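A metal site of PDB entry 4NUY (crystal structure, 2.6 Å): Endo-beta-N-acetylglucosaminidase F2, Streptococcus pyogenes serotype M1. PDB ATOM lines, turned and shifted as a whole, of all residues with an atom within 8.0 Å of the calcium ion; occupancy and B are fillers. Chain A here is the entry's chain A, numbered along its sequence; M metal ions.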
ATOM      1  N   ASN A 686     -11.969 -20.719 -29.040  1.00  0.00           N
ATOM      2  CA  ASN A 686     -13.216 -21.242 -29.588  1.00  0.00           C
ATOM      3  C   ASN A 686     -13.632 -22.520 -28.884  1.00  0.00           C
ATOM      4  O   ASN A 686     -14.820 -22.823 -28.783  1.00  0.00           O
ATOM      5  CB  ASN A 686     -13.094 -21.490 -31.096  1.00  0.00           C
ATOM      6  CG  ASN A 686     -13.240 -20.218 -31.898  1.00  0.00           C
ATOM      7  OD1 ASN A 686     -13.783 -19.221 -31.429  1.00  0.00           O
ATOM      8  ND2 ASN A 686     -12.767 -20.252 -33.143  1.00  0.00           N
ATOM      9  N   ALA A 687     -12.643 -23.269 -28.390  1.00  0.00           N
ATOM     10  CA  ALA A 687     -12.904 -24.487 -27.641  1.00  0.00           C
ATOM     11  C   ALA A 687     -13.667 -24.178 -26.353  1.00  0.00           C
ATOM     12  O   ALA A 687     -14.480 -24.970 -25.904  1.00  0.00           O
ATOM     13  CB  ALA A 687     -11.607 -25.213 -27.330  1.00  0.00           C
ATOM     14  N   ARG A 688     -13.396 -23.014 -25.772  1.00  0.00           N
ATOM     15  CA  ARG A 688     -14.065 -22.604 -24.543  1.00  0.00           C
ATOM     16  C   ARG A 688     -15.542 -22.290 -24.789  1.00  0.00           C
ATOM     17  O   ARG A 688     -16.334 -22.214 -23.848  1.00  0.00           O
ATOM     18  CB  ARG A 688     -13.361 -21.390 -23.925  1.00  0.00           C
ATOM     19  CG  ARG A 688     -12.037 -21.726 -23.271  1.00  0.00           C
ATOM     20  CD  ARG A 688     -11.485 -20.578 -22.440  1.00  0.00           C
ATOM     21  NE  ARG A 688     -11.006 -19.467 -23.267  1.00  0.00           N
ATOM     22  CZ  ARG A 688     -11.644 -18.305 -23.392  1.00  0.00           C
ATOM     23  NH1 ARG A 688     -12.779 -18.090 -22.743  1.00  0.00           N
ATOM     24  NH2 ARG A 688     -11.136 -17.351 -24.160  1.00  0.00           N
ATOM     25  N   LYS A 689     -15.893 -22.114 -26.056  1.00  0.00           N
ATOM     26  CA  LYS A 689     -17.255 -21.740 -26.425  1.00  0.00           C
ATOM     27  C   LYS A 689     -18.208 -22.934 -26.482  1.00  0.00           C
ATOM     28  O   LYS A 689     -19.418 -22.751 -26.604  1.00  0.00           O
ATOM     29  CB  LYS A 689     -17.262 -20.983 -27.756  1.00  0.00           C
ATOM     30  CG  LYS A 689     -16.449 -19.696 -27.721  1.00  0.00           C
ATOM     31  CD  LYS A 689     -16.347 -19.065 -29.099  1.00  0.00           C
ATOM     32  CE  LYS A 689     -15.633 -17.720 -29.040  1.00  0.00           C
ATOM     33  NZ  LYS A 689     -15.550 -17.107 -30.398  1.00  0.00           N
ATOM     34  N   VAL A 690     -17.661 -24.142 -26.393  1.00  0.00           N
ATOM     35  CA  VAL A 690     -18.507 -25.339 -26.325  1.00  0.00           C
ATOM     36  C   VAL A 690     -18.949 -25.581 -24.885  1.00  0.00           C
ATOM     37  O   VAL A 690     -19.708 -26.505 -24.602  1.00  0.00           O
ATOM     38  CB  VAL A 690     -17.794 -26.591 -26.863  1.00  0.00           C
ATOM     39  CG1 VAL A 690     -17.079 -26.291 -28.170  1.00  0.00           C
ATOM     40  CG2 VAL A 690     -16.811 -27.137 -25.823  1.00  0.00           C
ATOM     41  N   PHE A 691     -18.464 -24.739 -23.970  1.00  0.00           N
ATOM     42  CA  PHE A 691     -18.763 -24.896 -22.549  1.00  0.00           C
ATOM     43  C   PHE A 691     -19.394 -23.644 -21.964  1.00  0.00           C
ATOM     44  O   PHE A 691     -19.461 -23.512 -20.734  1.00  0.00           O
ATOM     45  CB  PHE A 691     -17.472 -25.220 -21.790  1.00  0.00           C
ATOM     46  CG  PHE A 691     -16.829 -26.511 -22.190  1.00  0.00           C
ATOM     47  CD1 PHE A 691     -17.570 -27.676 -22.292  1.00  0.00           C
ATOM     48  CD2 PHE A 691     -15.470 -26.554 -22.474  1.00  0.00           C
ATOM     49  CE1 PHE A 691     -16.976 -28.866 -22.660  1.00  0.00           C
ATOM     50  CE2 PHE A 691     -14.862 -27.746 -22.847  1.00  0.00           C
ATOM     51  CZ  PHE A 691     -15.613 -28.894 -22.936  1.00  0.00           C
ATOM     52  N   ASP A 692     -19.857 -22.730 -22.813  1.00  0.00           N
ATOM     53  CA  ASP A 692     -20.355 -21.444 -22.333  1.00  0.00           C
ATOM     54  C   ASP A 692     -21.850 -21.434 -21.977  1.00  0.00           C
ATOM     55  O   ASP A 692     -22.325 -20.507 -21.327  1.00  0.00           O
ATOM     56  CB  ASP A 692     -20.031 -20.315 -23.324  1.00  0.00           C
ATOM     57  CG  ASP A 692     -20.551 -20.572 -24.719  1.00  0.00           C
ATOM     58  OD1 ASP A 692     -21.404 -21.480 -24.889  1.00  0.00           O
ATOM     59  OD2 ASP A 692     -20.128 -19.867 -25.653  1.00  0.00           O
ATOM     60  N   GLY A 693     -22.570 -22.462 -22.396  1.00  0.00           N
ATOM     61  CA  GLY A 693     -23.973 -22.612 -22.034  1.00  0.00           C
ATOM     62  C   GLY A 693     -24.945 -21.984 -23.016  1.00  0.00           C
ATOM     63  O   GLY A 693     -26.124 -21.804 -22.699  1.00  0.00           O
ATOM     64  N   GLN A 694     -24.459 -21.657 -24.207  1.00  0.00           N
ATOM     65  CA  GLN A 694     -25.304 -21.087 -25.244  1.00  0.00           C
ATOM     66  C   GLN A 694     -24.984 -21.742 -26.581  1.00  0.00           C
ATOM     67  O   GLN A 694     -23.940 -22.363 -26.736  1.00  0.00           O
ATOM     68  CB  GLN A 694     -25.079 -19.583 -25.355  1.00  0.00           C
ATOM     69  CG  GLN A 694     -23.678 -19.212 -25.806  1.00  0.00           C
ATOM     70  CD  GLN A 694     -23.567 -17.754 -26.234  1.00  0.00           C
ATOM     71  OE1 GLN A 694     -22.588 -17.365 -26.866  1.00  0.00           O
ATOM     72  NE2 GLN A 694     -24.570 -16.963 -25.886  1.00  0.00           N
ATOM     73  N   LEU A 695     -25.889 -21.603 -27.547  1.00  0.00           N
ATOM     74  CA  LEU A 695     -25.635 -22.128 -28.893  1.00  0.00           C
ATOM     75  C   LEU A 695     -24.750 -21.155 -29.653  1.00  0.00           C
ATOM     76  O   LEU A 695     -24.223 -21.496 -30.717  1.00  0.00           O
ATOM     77  CB  LEU A 695     -26.955 -22.346 -29.638  1.00  0.00           C
ATOM     78  CG  LEU A 695     -27.839 -23.485 -29.129  1.00  0.00           C
ATOM     79  CD1 LEU A 695     -29.112 -23.573 -29.944  1.00  0.00           C
ATOM     80  CD2 LEU A 695     -27.072 -24.805 -29.182  1.00  0.00           C
ATOM     81  N   GLY A 696     -24.601 -19.958 -29.111  1.00  0.00           N
ATOM     82  CA  GLY A 696     -23.778 -18.937 -29.730  1.00  0.00           C
ATOM     83  C   GLY A 696     -24.557 -18.139 -30.762  1.00  0.00           C
ATOM     84  O   GLY A 696     -25.690 -18.485 -31.101  1.00  0.00           O
ATOM     85  N   SER A 697     -23.942 -17.074 -31.254  1.00  0.00           N
ATOM     86  CA  SER A 697     -24.550 -16.260 -32.293  1.00  0.00           C
ATOM     87  C   SER A 697     -24.248 -16.876 -33.652  1.00  0.00           C
ATOM     88  O   SER A 697     -23.201 -17.503 -33.839  1.00  0.00           O
ATOM     89  CB  SER A 697     -24.031 -14.830 -32.235  1.00  0.00           C
ATOM     90  OG  SER A 697     -24.680 -14.009 -33.198  1.00  0.00           O
ATOM     91  N   ASP A 700     -21.058 -15.630 -35.175  1.00  0.00           N
ATOM     92  CA  ASP A 700     -19.830 -15.901 -34.446  1.00  0.00           C
ATOM     93  C   ASP A 700     -19.002 -17.033 -35.054  1.00  0.00           C
ATOM     94  O   ASP A 700     -19.535 -18.095 -35.392  1.00  0.00           O
ATOM     95  CB  ASP A 700     -20.134 -16.200 -32.979  1.00  0.00           C
ATOM     96  CG  ASP A 700     -18.888 -16.298 -32.125  1.00  0.00           C
ATOM     97  OD1 ASP A 700     -17.872 -15.660 -32.479  1.00  0.00           O
ATOM     98  OD2 ASP A 700     -18.917 -17.007 -31.100  1.00  0.00           O
ATOM     99  N   ILE A 702     -16.972 -20.056 -34.634  1.00  0.00           N
ATOM    100  CA  ILE A 702     -16.953 -21.022 -33.551  1.00  0.00           C
ATOM    101  C   ILE A 702     -16.080 -22.243 -33.881  1.00  0.00           C
ATOM    102  O   ILE A 702     -15.893 -23.128 -33.039  1.00  0.00           O
ATOM    103  CB  ILE A 702     -18.391 -21.445 -33.153  1.00  0.00           C
ATOM    104  CG1 ILE A 702     -18.527 -21.554 -31.636  1.00  0.00           C
ATOM    105  CG2 ILE A 702     -18.806 -22.732 -33.848  1.00  0.00           C
ATOM    106  CD1 ILE A 702     -19.059 -20.290 -31.001  1.00  0.00           C
ATOM    107  N   PHE A 728     -23.633 -30.917 -29.938  1.00  0.00           N
ATOM    108  CA  PHE A 728     -24.489 -30.369 -30.978  1.00  0.00           C
ATOM    109  C   PHE A 728     -23.747 -30.164 -32.290  1.00  0.00           C
ATOM    110  O   PHE A 728     -22.534 -29.969 -32.306  1.00  0.00           O
ATOM    111  CB  PHE A 728     -25.074 -29.025 -30.510  1.00  0.00           C
ATOM    112  CG  PHE A 728     -25.958 -29.127 -29.295  1.00  0.00           C
ATOM    113  CD1 PHE A 728     -25.399 -29.166 -28.025  1.00  0.00           C
ATOM    114  CD2 PHE A 728     -27.333 -29.165 -29.431  1.00  0.00           C
ATOM    115  CE1 PHE A 728     -26.213 -29.251 -26.900  1.00  0.00           C
ATOM    116  CE2 PHE A 728     -28.144 -29.259 -28.318  1.00  0.00           C
ATOM    117  CZ  PHE A 728     -27.586 -29.297 -27.047  1.00  0.00           C
ATOM    118  N   ARG A 733     -27.523 -24.457 -34.185  1.00  0.00           N
ATOM    119  CA  ARG A 733     -27.405 -23.020 -34.077  1.00  0.00           C
ATOM    120  C   ARG A 733     -27.989 -22.358 -35.324  1.00  0.00           C
ATOM    121  O   ARG A 733     -28.717 -21.379 -35.239  1.00  0.00           O
ATOM    122  CB  ARG A 733     -25.936 -22.625 -33.936  1.00  0.00           C
ATOM    123  CG  ARG A 733     -25.706 -21.133 -33.822  1.00  0.00           C
ATOM    124  CD  ARG A 733     -24.234 -20.800 -33.906  1.00  0.00           C
ATOM    125  NE  ARG A 733     -23.647 -21.209 -35.182  1.00  0.00           N
ATOM    126  CZ  ARG A 733     -22.379 -20.993 -35.519  1.00  0.00           C
ATOM    127  NH1 ARG A 733     -21.563 -20.371 -34.691  1.00  0.00           N
ATOM    128  NH2 ARG A 733     -21.941 -21.395 -36.702  1.00  0.00           N
ATOM    129  N   VAL A 817     -18.760 -27.182 -33.492  1.00  0.00           N
ATOM    130  CA  VAL A 817     -19.588 -27.672 -32.392  1.00  0.00           C
ATOM    131  C   VAL A 817     -20.007 -26.547 -31.463  1.00  0.00           C
ATOM    132  O   VAL A 817     -19.184 -26.017 -30.708  1.00  0.00           O
ATOM    133  CB  VAL A 817     -18.839 -28.736 -31.562  1.00  0.00           C
ATOM    134  CG1 VAL A 817     -19.736 -29.287 -30.450  1.00  0.00           C
ATOM    135  CG2 VAL A 817     -18.349 -29.870 -32.450  1.00  0.00           C
ATOM    136  N   PRO A 818     -21.293 -26.162 -31.507  1.00  0.00           N
ATOM    137  CA  PRO A 818     -21.834 -25.091 -30.667  1.00  0.00           C
ATOM    138  C   PRO A 818     -21.731 -25.377 -29.169  1.00  0.00           C
ATOM    139  O   PRO A 818     -21.482 -24.452 -28.401  1.00  0.00           O
ATOM    140  CB  PRO A 818     -23.303 -25.012 -31.100  1.00  0.00           C
ATOM    141  CG  PRO A 818     -23.316 -25.564 -32.480  1.00  0.00           C
ATOM    142  CD  PRO A 818     -22.293 -26.659 -32.475  1.00  0.00           C
ATOM    143  N   GLU A 819     -21.936 -26.621 -28.765  1.00  0.00           N
ATOM    144  CA  GLU A 819     -21.906 -26.960 -27.341  1.00  0.00           C
ATOM    145  C   GLU A 819     -21.563 -28.429 -27.097  1.00  0.00           C
ATOM    146  O   GLU A 819     -21.979 -29.315 -27.836  1.00  0.00           O
ATOM    147  CB  GLU A 819     -23.256 -26.651 -26.688  1.00  0.00           C
ATOM    148  CG  GLU A 819     -23.314 -25.326 -25.946  1.00  0.00           C
ATOM    149  CD  GLU A 819     -22.635 -25.376 -24.597  1.00  0.00           C
ATOM    150  OE1 GLU A 819     -22.859 -26.350 -23.847  1.00  0.00           O
ATOM    151  OE2 GLU A 819     -21.885 -24.430 -24.270  1.00  0.00           O
ATOM    152  N   LEU A 820     -20.792 -28.670 -26.036  1.00  0.00           N
ATOM    153  CA  LEU A 820     -20.561 -30.014 -25.551  1.00  0.00           C
ATOM    154  C   LEU A 820     -21.088 -30.104 -24.117  1.00  0.00           C
ATOM    155  O   LEU A 820     -20.717 -29.311 -23.262  1.00  0.00           O
ATOM    156  CB  LEU A 820     -19.076 -30.377 -25.588  1.00  0.00           C
ATOM    157  CG  LEU A 820     -18.714 -31.721 -24.955  1.00  0.00           C
ATOM    158  CD1 LEU A 820     -19.487 -32.872 -25.593  1.00  0.00           C
ATOM    159  CD2 LEU A 820     -17.212 -31.985 -25.036  1.00  0.00           C
HETATM  160 CA    CA M   1     -21.670 -22.317 -27.407  1.00  0.00          CA
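The side-chain amide oxygen of Asn 686 is in hydrogen-bond range of the side-chain amino group of Lys 689 (2.9 Å).
OD1 of Asp 700 lies within salt-bridge range of NZ of Lys 689, at 3.4 Å.
OE2 of Glu 819 sits at hydrogen-bond distance from N of Asp 692, at 3.0 Å.
N of Gly 693 sits at hydrogen-bond distance from OE2 of Glu 819.
OE2 of Glu 819 is in hydrogen-bond range of N of Phe 691 (3.4 Å).
O of Glu 819 sits at hydrogen-bond distance from N of Phe 728 (3.1 Å).
Leu 695 touches the calcium ion (C to CA, 3.99 Å).
Glu 819 touches the calcium ion.
Of the 20 residues printed, 6 come within 4 Å of the calcium ion.
The calcium ion is bound by the backbone carbonyl oxygen (O) of Pro 818 (2.4 Å).
The calcium ion is bound by O of Gln 694, 2.4 Å away.
The backbone carbonyl oxygen (O) of Lys 689 binds the calcium ion (2.4 Å).
The side-chain carboxylate (OD1) of Asp 692 is bound to the calcium ion (2.7 Å).
The calcium ion has four donor atoms within binding distance.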
